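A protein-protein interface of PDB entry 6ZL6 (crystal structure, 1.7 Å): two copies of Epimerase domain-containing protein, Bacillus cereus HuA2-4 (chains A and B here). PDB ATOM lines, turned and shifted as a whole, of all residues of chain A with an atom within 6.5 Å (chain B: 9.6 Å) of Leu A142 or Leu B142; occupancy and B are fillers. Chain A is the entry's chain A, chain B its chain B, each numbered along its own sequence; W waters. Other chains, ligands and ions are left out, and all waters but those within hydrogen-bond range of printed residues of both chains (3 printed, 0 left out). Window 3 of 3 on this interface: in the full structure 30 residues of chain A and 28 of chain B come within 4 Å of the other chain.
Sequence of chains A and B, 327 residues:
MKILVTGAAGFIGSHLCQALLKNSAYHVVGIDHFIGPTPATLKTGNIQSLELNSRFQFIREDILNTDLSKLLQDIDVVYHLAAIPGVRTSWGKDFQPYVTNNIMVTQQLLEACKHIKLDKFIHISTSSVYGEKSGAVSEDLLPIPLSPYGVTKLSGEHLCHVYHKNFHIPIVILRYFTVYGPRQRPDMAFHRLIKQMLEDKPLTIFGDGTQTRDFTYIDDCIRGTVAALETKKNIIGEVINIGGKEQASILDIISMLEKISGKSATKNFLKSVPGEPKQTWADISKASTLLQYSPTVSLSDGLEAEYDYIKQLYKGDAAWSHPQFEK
The backbone carbonyl oxygen (O) of Tyr A130 sits at hydrogen-bond distance from the backbone NH (N) of Ile A144, 3.2 Å away. The side-chain amino group of Lys A133 sits at hydrogen-bond distance from the backbone carbonyl oxygen of Leu A142 (2.6 Å).
Leu B142 touches Leu A142. Pro B143 touches Leu A142. Pro A143 touches Leu B142 (CD to CD1, 3.4 Å). NZ of Lys B165 touches CG2 of Ile A144, at 3.6 Å. NE2 of His A158 touches O of Pro B143 (3.8 Å). Leu B154 touches His A158.
Of the 11 printed residues of chain A, 4 touch a printed residue of chain B. Printed residues of chain A that touch a printed residue of chain B: Leu A142, Pro A143, Ile A144 and His A158. Hydrophobic or aromatic side chains of chain A within 4 Å of the printed part of chain B: Leu A142, Pro A143, Ile A144 and His A158. Of the 23 printed residues of chain B, 4 touch a printed residue of chain A. Hydrophobic or aromatic side chains of chain B within 4 Å of the printed part of chain A: Leu B142, Pro B143 and Leu B154. Among the printed residues, 6 pairs touch across the chains.
Water W2 lies within hydrogen-bond range of O of His A158 and O of Pro B145. Water W1 bridges O of Pro B143 and NE2 of His A158. Water W3 bridges the backbone carbonyl oxygen of Pro A143 (2.8 Å) and a ring nitrogen (NE2) of His B158 (3.0 Å).
Leu B142 touches its own counterpart, Leu A142. Leu A142 touches Pro B143, and with the chains exchanged Pro A143 touches Leu B142. His A158 touches Pro B143, but with the chains exchanged Pro A143 does not touch His B158 (4.1 Å). 11 positions are printed for both chains.
Of chain A, only Leu A142 (3.9 Å) and Pro A143 (3.4 Å) come within 4 Å of Leu B142. No residue of chain B comes within 4 Å of Leu A141. Printed residues of chain A within 4 Å of Leu B154: His A158. Of the printed residues of chain B, Ile A144 touches Lys B165 (3.6 Å). Of the printed residues of chain A, Pro B143 touches Leu A142 (3.7 Å) and His A158 (3.8 Å). Of the printed residues of chain A, Lys B165 touches Ile A144 (3.6 Å). Printed residues of chain B within 4 Å of His A158: Pro B143 (3.8 Å) and Leu B154 (3.2 Å).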
ATOM      1  N   VAL A 129     -41.071 -19.177  16.721  1.00  0.00           N
ATOM      2  CA  VAL A 129     -39.666 -18.844  16.373  1.00  0.00           C
ATOM      3  C   VAL A 129     -39.005 -18.164  17.566  1.00  0.00           C
ATOM      4  O   VAL A 129     -37.770 -18.261  17.634  1.00  0.00           O
ATOM      5  CB  VAL A 129     -39.525 -18.022  15.086  1.00  0.00           C
ATOM      6  CG1 VAL A 129     -40.140 -18.758  13.896  1.00  0.00           C
ATOM      7  CG2 VAL A 129     -40.086 -16.628  15.221  1.00  0.00           C
ATOM      8  N   TYR A 130     -39.768 -17.511  18.440  1.00  0.00           N
ATOM      9  CA  TYR A 130     -39.189 -16.656  19.494  1.00  0.00           C
ATOM     10  C   TYR A 130     -38.529 -17.558  20.532  1.00  0.00           C
ATOM     11  O   TYR A 130     -37.473 -17.189  21.055  1.00  0.00           O
ATOM     12  CB  TYR A 130     -40.193 -15.712  20.135  1.00  0.00           C
ATOM     13  CG  TYR A 130     -40.608 -14.566  19.249  1.00  0.00           C
ATOM     14  CD1 TYR A 130     -39.758 -13.512  18.982  1.00  0.00           C
ATOM     15  CD2 TYR A 130     -41.883 -14.515  18.722  1.00  0.00           C
ATOM     16  CE1 TYR A 130     -40.165 -12.425  18.228  1.00  0.00           C
ATOM     17  CE2 TYR A 130     -42.309 -13.441  17.966  1.00  0.00           C
ATOM     18  CZ  TYR A 130     -41.434 -12.407  17.685  1.00  0.00           C
ATOM     19  OH  TYR A 130     -41.855 -11.344  16.917  1.00  0.00           O
ATOM     20  N   LYS A 133     -39.362 -16.297  25.983  1.00  0.00           N
ATOM     21  CA  LYS A 133     -39.070 -14.860  26.196  1.00  0.00           C
ATOM     22  C   LYS A 133     -40.061 -14.303  27.199  1.00  0.00           C
ATOM     23  O   LYS A 133     -41.242 -14.755  27.254  1.00  0.00           O
ATOM     24  CB  LYS A 133     -39.173 -14.012  24.921  1.00  0.00           C
ATOM     25  CG  LYS A 133     -38.369 -14.487  23.724  1.00  0.00           C
ATOM     26  CD  LYS A 133     -36.874 -14.251  23.803  1.00  0.00           C
ATOM     27  CE  LYS A 133     -36.232 -14.610  22.477  1.00  0.00           C
ATOM     28  NZ  LYS A 133     -34.783 -14.361  22.452  1.00  0.00           N
ATOM     29  N   SER A 138     -41.373  -8.069  20.560  1.00  0.00           N
ATOM     30  CA  SER A 138     -41.342  -7.254  19.337  1.00  0.00           C
ATOM     31  C   SER A 138     -40.581  -8.028  18.253  1.00  0.00           C
ATOM     32  O   SER A 138     -39.820  -8.971  18.548  1.00  0.00           O
ATOM     33  CB  SER A 138     -40.765  -5.884  19.609  1.00  0.00           C
ATOM     34  OG  SER A 138     -39.451  -6.025  20.063  1.00  0.00           O
ATOM     35  N   GLU A 139     -40.781  -7.630  17.002  1.00  0.00           N
ATOM     36  CA  GLU A 139     -40.289  -8.381  15.830  1.00  0.00           C
ATOM     37  C   GLU A 139     -38.779  -8.194  15.625  1.00  0.00           C
ATOM     38  O   GLU A 139     -38.231  -8.936  14.811  1.00  0.00           O
ATOM     39  CB  GLU A 139     -41.081  -7.900  14.619  1.00  0.00           C
ATOM     40  CG  GLU A 139     -42.588  -8.153  14.697  1.00  0.00           C
ATOM     41  CD  GLU A 139     -43.451  -7.035  15.262  1.00  0.00           C
ATOM     42  OE1 GLU A 139     -42.893  -6.104  15.914  1.00  0.00           O
ATOM     43  OE2 GLU A 139     -44.672  -7.116  15.103  1.00  0.00           O
ATOM     44  N   ASP A 140     -38.118  -7.261  16.341  1.00  0.00           N
ATOM     45  CA  ASP A 140     -36.653  -7.031  16.248  1.00  0.00           C
ATOM     46  C   ASP A 140     -35.897  -7.896  17.258  1.00  0.00           C
ATOM     47  O   ASP A 140     -34.661  -7.871  17.248  1.00  0.00           O
ATOM     48  CB  ASP A 140     -36.330  -5.538  16.377  1.00  0.00           C
ATOM     49  CG  ASP A 140     -37.054  -4.853  17.534  1.00  0.00           C
ATOM     50  OD1 ASP A 140     -37.648  -5.584  18.356  1.00  0.00           O
ATOM     51  OD2 ASP A 140     -36.975  -3.600  17.636  1.00  0.00           O
ATOM     52  N   LEU A 141     -36.589  -8.726  18.037  1.00  0.00           N
ATOM     53  CA  LEU A 141     -35.970  -9.562  19.087  1.00  0.00           C
ATOM     54  C   LEU A 141     -35.283 -10.794  18.481  1.00  0.00           C
ATOM     55  O   LEU A 141     -35.867 -11.432  17.595  1.00  0.00           O
ATOM     56  CB  LEU A 141     -37.146  -9.891  19.992  1.00  0.00           C
ATOM     57  CG  LEU A 141     -36.899 -10.483  21.362  1.00  0.00           C
ATOM     58  CD1 LEU A 141     -35.733  -9.818  22.088  1.00  0.00           C
ATOM     59  CD2 LEU A 141     -38.178 -10.329  22.145  1.00  0.00           C
ATOM     60  N   LEU A 142     -34.102 -11.165  18.975  1.00  0.00           N
ATOM     61  CA  LEU A 142     -33.319 -12.324  18.494  1.00  0.00           C
ATOM     62  C   LEU A 142     -34.108 -13.608  18.748  1.00  0.00           C
ATOM     63  O   LEU A 142     -34.352 -13.960  19.896  1.00  0.00           O
ATOM     64  CB  LEU A 142     -31.973 -12.356  19.225  1.00  0.00           C
ATOM     65  CG  LEU A 142     -31.180 -13.657  19.085  1.00  0.00           C
ATOM     66  CD1 LEU A 142     -30.554 -13.726  17.715  1.00  0.00           C
ATOM     67  CD2 LEU A 142     -30.089 -13.775  20.157  1.00  0.00           C
ATOM     68  N   PRO A 143     -34.592 -14.317  17.700  1.00  0.00           N
ATOM     69  CA  PRO A 143     -35.345 -15.550  17.889  1.00  0.00           C
ATOM     70  C   PRO A 143     -34.436 -16.705  18.303  1.00  0.00           C
ATOM     71  O   PRO A 143     -33.435 -16.897  17.657  1.00  0.00           O
ATOM     72  CB  PRO A 143     -35.909 -15.891  16.487  1.00  0.00           C
ATOM     73  CG  PRO A 143     -35.672 -14.663  15.647  1.00  0.00           C
ATOM     74  CD  PRO A 143     -34.467 -13.983  16.275  1.00  0.00           C
ATOM     75  N   ILE A 144     -34.803 -17.431  19.355  1.00  0.00           N
ATOM     76  CA  ILE A 144     -34.126 -18.699  19.739  1.00  0.00           C
ATOM     77  C   ILE A 144     -35.199 -19.748  19.955  1.00  0.00           C
ATOM     78  O   ILE A 144     -35.741 -19.892  21.054  1.00  0.00           O
ATOM     79  CB  ILE A 144     -33.200 -18.529  20.961  1.00  0.00           C
ATOM     80  CG1 ILE A 144     -32.204 -17.381  20.751  1.00  0.00           C
ATOM     81  CG2 ILE A 144     -32.472 -19.839  21.285  1.00  0.00           C
ATOM     82  CD1 ILE A 144     -31.234 -17.600  19.578  1.00  0.00           C
ATOM     83  N   HIS A 158     -36.246 -17.212   6.950  1.00  0.00           N
ATOM     84  CA  HIS A 158     -34.873 -16.880   6.483  1.00  0.00           C
ATOM     85  C   HIS A 158     -34.805 -17.079   4.974  1.00  0.00           C
ATOM     86  O   HIS A 158     -34.213 -16.177   4.295  1.00  0.00           O
ATOM     87  CB  HIS A 158     -33.816 -17.672   7.249  1.00  0.00           C
ATOM     88  CG  HIS A 158     -33.625 -17.248   8.664  1.00  0.00           C
ATOM     89  ND1 HIS A 158     -33.137 -18.125   9.605  1.00  0.00           N
ATOM     90  CD2 HIS A 158     -33.888 -16.096   9.313  1.00  0.00           C
ATOM     91  CE1 HIS A 158     -33.031 -17.489  10.764  1.00  0.00           C
ATOM     92  NE2 HIS A 158     -33.502 -16.266  10.612  1.00  0.00           N
ATOM     93  N   SER B 127     -19.642 -17.917   9.320  1.00  0.00           N
ATOM     94  CA  SER B 127     -19.957 -16.474   9.207  1.00  0.00           C
ATOM     95  C   SER B 127     -21.137 -16.260   8.268  1.00  0.00           C
ATOM     96  O   SER B 127     -21.771 -15.157   8.318  1.00  0.00           O
ATOM     97  CB  SER B 127     -18.769 -15.676   8.745  1.00  0.00           C
ATOM     98  OG  SER B 127     -18.266 -16.200   7.516  1.00  0.00           O
ATOM     99  N   SER B 128     -21.492 -17.268   7.470  1.00  0.00           N
ATOM    100  CA  SER B 128     -22.550 -17.108   6.466  1.00  0.00           C
ATOM    101  C   SER B 128     -23.905 -16.996   7.158  1.00  0.00           C
ATOM    102  O   SER B 128     -24.868 -16.655   6.444  1.00  0.00           O
ATOM    103  CB  SER B 128     -22.544 -18.201   5.415  1.00  0.00           C
ATOM    104  OG  SER B 128     -21.351 -18.156   4.681  1.00  0.00           O
ATOM    105  N   VAL B 129     -24.010 -17.261   8.460  1.00  0.00           N
ATOM    106  CA  VAL B 129     -25.312 -17.069   9.159  1.00  0.00           C
ATOM    107  C   VAL B 129     -25.616 -15.563   9.315  1.00  0.00           C
ATOM    108  O   VAL B 129     -26.772 -15.222   9.442  1.00  0.00           O
ATOM    109  CB  VAL B 129     -25.367 -17.818  10.495  1.00  0.00           C
ATOM    110  CG1 VAL B 129     -25.053 -19.310  10.315  1.00  0.00           C
ATOM    111  CG2 VAL B 129     -24.477 -17.171  11.523  1.00  0.00           C
ATOM    112  N   TYR B 130     -24.622 -14.681   9.279  1.00  0.00           N
ATOM    113  CA  TYR B 130     -24.843 -13.259   9.618  1.00  0.00           C
ATOM    114  C   TYR B 130     -25.447 -12.489   8.436  1.00  0.00           C
ATOM    115  O   TYR B 130     -26.254 -11.568   8.654  1.00  0.00           O
ATOM    116  CB  TYR B 130     -23.536 -12.584   9.998  1.00  0.00           C
ATOM    117  CG  TYR B 130     -22.971 -13.026  11.318  1.00  0.00           C
ATOM    118  CD1 TYR B 130     -23.549 -12.618  12.510  1.00  0.00           C
ATOM    119  CD2 TYR B 130     -21.815 -13.779  11.388  1.00  0.00           C
ATOM    120  CE1 TYR B 130     -23.014 -12.989  13.732  1.00  0.00           C
ATOM    121  CE2 TYR B 130     -21.263 -14.160  12.600  1.00  0.00           C
ATOM    122  CZ  TYR B 130     -21.859 -13.755  13.784  1.00  0.00           C
ATOM    123  OH  TYR B 130     -21.340 -14.114  15.006  1.00  0.00           O
ATOM    124  N   GLY B 131     -24.958 -12.729   7.231  1.00  0.00           N
ATOM    125  CA  GLY B 131     -25.241 -11.794   6.121  1.00  0.00           C
ATOM    126  C   GLY B 131     -24.456 -10.498   6.300  1.00  0.00           C
ATOM    127  O   GLY B 131     -23.254 -10.605   6.613  1.00  0.00           O
ATOM    128  N   GLU B 132     -25.094  -9.319   6.217  1.00  0.00           N
ATOM    129  CA  GLU B 132     -24.387  -8.039   5.901  1.00  0.00           C
ATOM    130  C   GLU B 132     -24.434  -7.002   7.031  1.00  0.00           C
ATOM    131  O   GLU B 132     -25.542  -6.500   7.293  1.00  0.00           O
ATOM    132  CB  GLU B 132     -25.003  -7.427   4.640  1.00  0.00           C
ATOM    133  CG  GLU B 132     -24.061  -6.492   3.919  1.00  0.00           C
ATOM    134  CD  GLU B 132     -22.929  -7.172   3.160  1.00  0.00           C
ATOM    135  OE1 GLU B 132     -23.195  -7.711   2.065  1.00  0.00           O
ATOM    136  OE2 GLU B 132     -21.774  -7.123   3.655  1.00  0.00           O
ATOM    137  N   LYS B 133     -23.267  -6.582   7.565  1.00  0.00           N
ATOM    138  CA  LYS B 133     -23.160  -5.568   8.652  1.00  0.00           C
ATOM    139  C   LYS B 133     -21.944  -4.636   8.488  1.00  0.00           C
ATOM    140  O   LYS B 133     -20.985  -5.004   7.839  1.00  0.00           O
ATOM    141  CB  LYS B 133     -23.094  -6.302   9.995  1.00  0.00           C
ATOM    142  CG  LYS B 133     -24.273  -7.225  10.276  1.00  0.00           C
ATOM    143  CD  LYS B 133     -25.575  -6.474  10.537  1.00  0.00           C
ATOM    144  CE  LYS B 133     -26.746  -7.372  10.891  1.00  0.00           C
ATOM    145  NZ  LYS B 133     -27.175  -8.211   9.746  1.00  0.00           N
ATOM    146  N   VAL B 137     -18.771  -8.247  13.584  1.00  0.00           N
ATOM    147  CA  VAL B 137     -20.049  -8.793  14.119  1.00  0.00           C
ATOM    148  C   VAL B 137     -19.808  -9.602  15.401  1.00  0.00           C
ATOM    149  O   VAL B 137     -18.872 -10.462  15.478  1.00  0.00           O
ATOM    150  CB  VAL B 137     -20.810  -9.620  13.068  1.00  0.00           C
ATOM    151  CG1 VAL B 137     -21.251  -8.758  11.902  1.00  0.00           C
ATOM    152  CG2 VAL B 137     -20.003 -10.803  12.561  1.00  0.00           C
ATOM    153  N   SER B 138     -20.657  -9.332  16.387  1.00  0.00           N
ATOM    154  CA  SER B 138     -20.708 -10.077  17.659  1.00  0.00           C
ATOM    155  C   SER B 138     -21.667 -11.253  17.528  1.00  0.00           C
ATOM    156  O   SER B 138     -22.631 -11.199  16.714  1.00  0.00           O
ATOM    157  CB  SER B 138     -21.126  -9.174  18.801  1.00  0.00           C
ATOM    158  OG  SER B 138     -20.027  -8.391  19.175  1.00  0.00           O
ATOM    159  N   GLU B 139     -21.471 -12.251  18.380  1.00  0.00           N
ATOM    160  CA  GLU B 139     -22.266 -13.507  18.342  1.00  0.00           C
ATOM    161  C   GLU B 139     -23.712 -13.258  18.779  1.00  0.00           C
ATOM    162  O   GLU B 139     -24.548 -14.106  18.491  1.00  0.00           O
ATOM    163  CB  GLU B 139     -21.601 -14.542  19.239  1.00  0.00           C
ATOM    164  CG  GLU B 139     -20.180 -14.885  18.798  1.00  0.00           C
ATOM    165  CD  GLU B 139     -18.996 -14.100  19.323  1.00  0.00           C
ATOM    166  OE1 GLU B 139     -19.186 -13.006  19.904  1.00  0.00           O
ATOM    167  OE2 GLU B 139     -17.872 -14.584  19.141  1.00  0.00           O
ATOM    168  N   ASP B 140     -23.984 -12.127  19.442  1.00  0.00           N
ATOM    169  CA  ASP B 140     -25.320 -11.721  19.954  1.00  0.00           C
ATOM    170  C   ASP B 140     -26.096 -10.923  18.891  1.00  0.00           C
ATOM    171  O   ASP B 140     -27.266 -10.644  19.124  1.00  0.00           O
ATOM    172  CB  ASP B 140     -25.208 -10.974  21.294  1.00  0.00           C
ATOM    173  CG  ASP B 140     -24.092  -9.941  21.370  1.00  0.00           C
ATOM    174  OD1 ASP B 140     -22.909 -10.344  21.457  1.00  0.00           O
ATOM    175  OD2 ASP B 140     -24.406  -8.737  21.380  1.00  0.00           O
ATOM    176  N   LEU B 141     -25.533 -10.705  17.707  1.00  0.00           N
ATOM    177  CA  LEU B 141     -26.211  -9.971  16.611  1.00  0.00           C
ATOM    178  C   LEU B 141     -27.273 -10.868  15.948  1.00  0.00           C
ATOM    179  O   LEU B 141     -26.958 -12.033  15.665  1.00  0.00           O
ATOM    180  CB  LEU B 141     -25.120  -9.546  15.635  1.00  0.00           C
ATOM    181  CG  LEU B 141     -25.558  -8.693  14.461  1.00  0.00           C
ATOM    182  CD1 LEU B 141     -26.188  -7.377  14.932  1.00  0.00           C
ATOM    183  CD2 LEU B 141     -24.339  -8.445  13.580  1.00  0.00           C
ATOM    184  N   LEU B 142     -28.478 -10.325  15.715  1.00  0.00           N
ATOM    185  CA  LEU B 142     -29.582 -10.964  14.957  1.00  0.00           C
ATOM    186  C   LEU B 142     -29.046 -11.405  13.606  1.00  0.00           C
ATOM    187  O   LEU B 142     -28.688 -10.575  12.776  1.00  0.00           O
ATOM    188  CB  LEU B 142     -30.739  -9.981  14.757  1.00  0.00           C
ATOM    189  CG  LEU B 142     -31.889 -10.529  13.908  1.00  0.00           C
ATOM    190  CD1 LEU B 142     -32.748 -11.446  14.746  1.00  0.00           C
ATOM    191  CD2 LEU B 142     -32.738  -9.402  13.326  1.00  0.00           C
ATOM    192  N   PRO B 143     -28.930 -12.723  13.359  1.00  0.00           N
ATOM    193  CA  PRO B 143     -28.418 -13.227  12.094  1.00  0.00           C
ATOM    194  C   PRO B 143     -29.551 -13.355  11.073  1.00  0.00           C
ATOM    195  O   PRO B 143     -30.558 -13.915  11.404  1.00  0.00           O
ATOM    196  CB  PRO B 143     -27.837 -14.589  12.510  1.00  0.00           C
ATOM    197  CG  PRO B 143     -28.792 -15.066  13.562  1.00  0.00           C
ATOM    198  CD  PRO B 143     -29.268 -13.816  14.282  1.00  0.00           C
ATOM    199  N   ILE B 144     -29.325 -12.806   9.880  1.00  0.00           N
ATOM    200  CA  ILE B 144     -30.179 -12.917   8.675  1.00  0.00           C
ATOM    201  C   ILE B 144     -29.298 -13.335   7.509  1.00  0.00           C
ATOM    202  O   ILE B 144     -28.582 -12.515   6.896  1.00  0.00           O
ATOM    203  CB  ILE B 144     -30.964 -11.621   8.404  1.00  0.00           C
ATOM    204  CG1 ILE B 144     -31.752 -11.181   9.639  1.00  0.00           C
ATOM    205  CG2 ILE B 144     -31.880 -11.829   7.226  1.00  0.00           C
ATOM    206  CD1 ILE B 144     -32.881 -12.122  10.025  1.00  0.00           C
ATOM    207  N   PRO B 145     -29.251 -14.670   7.253  1.00  0.00           N
ATOM    208  CA  PRO B 145     -28.433 -15.205   6.176  1.00  0.00           C
ATOM    209  C   PRO B 145     -28.794 -14.542   4.840  1.00  0.00           C
ATOM    210  O   PRO B 145     -29.968 -14.189   4.625  1.00  0.00           O
ATOM    211  CB  PRO B 145     -28.775 -16.702   6.158  1.00  0.00           C
ATOM    212  CG  PRO B 145     -29.182 -17.013   7.579  1.00  0.00           C
ATOM    213  CD  PRO B 145     -29.858 -15.739   8.072  1.00  0.00           C
ATOM    214  N   LEU B 154     -27.562 -22.025   9.806  1.00  0.00           N
ATOM    215  CA  LEU B 154     -28.178 -21.372  10.977  1.00  0.00           C
ATOM    216  C   LEU B 154     -29.244 -22.331  11.539  1.00  0.00           C
ATOM    217  O   LEU B 154     -29.385 -22.418  12.726  1.00  0.00           O
ATOM    218  CB  LEU B 154     -28.729 -19.997  10.584  1.00  0.00           C
ATOM    219  CG  LEU B 154     -29.354 -19.211  11.728  1.00  0.00           C
ATOM    220  CD1 LEU B 154     -28.374 -19.042  12.883  1.00  0.00           C
ATOM    221  CD2 LEU B 154     -29.882 -17.868  11.216  1.00  0.00           C
ATOM    222  N   GLU B 157     -27.445 -24.668  13.875  1.00  0.00           N
ATOM    223  CA  GLU B 157     -27.184 -23.982  15.158  1.00  0.00           C
ATOM    224  C   GLU B 157     -28.438 -24.049  16.020  1.00  0.00           C
ATOM    225  O   GLU B 157     -28.372 -24.436  17.190  1.00  0.00           O
ATOM    226  CB  GLU B 157     -26.833 -22.509  14.999  1.00  0.00           C
ATOM    227  CG  GLU B 157     -25.520 -22.250  14.301  1.00  0.00           C
ATOM    228  CD  GLU B 157     -24.977 -20.828  14.459  1.00  0.00           C
ATOM    229  OE1 GLU B 157     -25.450 -20.145  15.390  1.00  0.00           O
ATOM    230  OE2 GLU B 157     -24.037 -20.420  13.679  1.00  0.00           O
ATOM    231  N   HIS B 158     -29.575 -23.675  15.448  1.00  0.00           N
ATOM    232  CA  HIS B 158     -30.834 -23.653  16.217  1.00  0.00           C
ATOM    233  C   HIS B 158     -31.210 -25.033  16.736  1.00  0.00           C
ATOM    234  O   HIS B 158     -31.681 -25.113  17.896  1.00  0.00           O
ATOM    235  CB  HIS B 158     -31.941 -23.068  15.363  1.00  0.00           C
ATOM    236  CG  HIS B 158     -31.786 -21.616  15.165  1.00  0.00           C
ATOM    237  ND1 HIS B 158     -32.304 -20.977  14.042  1.00  0.00           N
ATOM    238  CD2 HIS B 158     -31.134 -20.674  15.865  1.00  0.00           C
ATOM    239  CE1 HIS B 158     -32.002 -19.692  14.120  1.00  0.00           C
ATOM    240  NE2 HIS B 158     -31.315 -19.478  15.206  1.00  0.00           N
ATOM    241  N   HIS B 161     -29.294 -25.573  19.927  1.00  0.00           N
ATOM    242  CA  HIS B 161     -29.902 -24.831  21.064  1.00  0.00           C
ATOM    243  C   HIS B 161     -31.088 -25.635  21.586  1.00  0.00           C
ATOM    244  O   HIS B 161     -31.200 -25.830  22.797  1.00  0.00           O
ATOM    245  CB  HIS B 161     -30.318 -23.412  20.694  1.00  0.00           C
ATOM    246  CG  HIS B 161     -29.145 -22.518  20.425  1.00  0.00           C
ATOM    247  ND1 HIS B 161     -28.128 -22.340  21.366  1.00  0.00           N
ATOM    248  CD2 HIS B 161     -28.822 -21.748  19.352  1.00  0.00           C
ATOM    249  CE1 HIS B 161     -27.230 -21.493  20.886  1.00  0.00           C
ATOM    250  NE2 HIS B 161     -27.640 -21.115  19.647  1.00  0.00           N
ATOM    251  N   LYS B 165     -31.182 -27.191  25.376  1.00  0.00           N
ATOM    252  CA  LYS B 165     -32.138 -26.718  26.420  1.00  0.00           C
ATOM    253  C   LYS B 165     -33.041 -27.881  26.860  1.00  0.00           C
ATOM    254  O   LYS B 165     -33.337 -27.962  28.058  1.00  0.00           O
ATOM    255  CB  LYS B 165     -32.915 -25.500  25.932  1.00  0.00           C
ATOM    256  CG  LYS B 165     -32.082 -24.251  25.707  1.00  0.00           C
ATOM    257  CD  LYS B 165     -32.796 -23.253  24.786  1.00  0.00           C
ATOM    258  CE  LYS B 165     -31.878 -22.350  23.982  1.00  0.00           C
ATOM    259  NZ  LYS B 165     -31.753 -21.033  24.638  1.00  0.00           N
ATOM    260  N   ARG B 175     -18.365 -20.367  15.011  1.00  0.00           N
ATOM    261  CA  ARG B 175     -18.655 -19.807  13.682  1.00  0.00           C
ATOM    262  C   ARG B 175     -17.324 -19.486  13.023  1.00  0.00           C
ATOM    263  O   ARG B 175     -16.694 -18.501  13.433  1.00  0.00           O
ATOM    264  CB  ARG B 175     -19.544 -18.580  13.799  1.00  0.00           C
ATOM    265  CG  ARG B 175     -20.950 -18.892  14.231  1.00  0.00           C
ATOM    266  CD  ARG B 175     -21.720 -17.590  14.423  1.00  0.00           C
ATOM    267  NE  ARG B 175     -23.111 -17.882  14.661  1.00  0.00           N
ATOM    268  CZ  ARG B 175     -24.019 -17.038  15.161  1.00  0.00           C
ATOM    269  NH1 ARG B 175     -23.678 -15.797  15.427  1.00  0.00           N
ATOM    270  NH2 ARG B 175     -25.276 -17.423  15.341  1.00  0.00           N
ATOM    271  N   VAL B 239     -21.976 -19.420  21.632  1.00  0.00           N
ATOM    272  CA  VAL B 239     -21.629 -19.265  20.190  1.00  0.00           C
ATOM    273  C   VAL B 239     -20.334 -18.449  20.146  1.00  0.00           C
ATOM    274  O   VAL B 239     -20.270 -17.410  20.831  1.00  0.00           O
ATOM    275  CB  VAL B 239     -22.781 -18.591  19.434  1.00  0.00           C
ATOM    276  CG1 VAL B 239     -22.422 -18.357  17.977  1.00  0.00           C
ATOM    277  CG2 VAL B 239     -24.077 -19.369  19.572  1.00  0.00           C
HETATM  278  O   HOH W   1     -32.627 -14.872  13.044  1.00  0.00           O
HETATM  279  O   HOH W   2     -32.322 -15.018   5.879  1.00  0.00           O
HETATM  280  O   HOH W   3     -31.385 -16.496  15.771  1.00  0.00           O
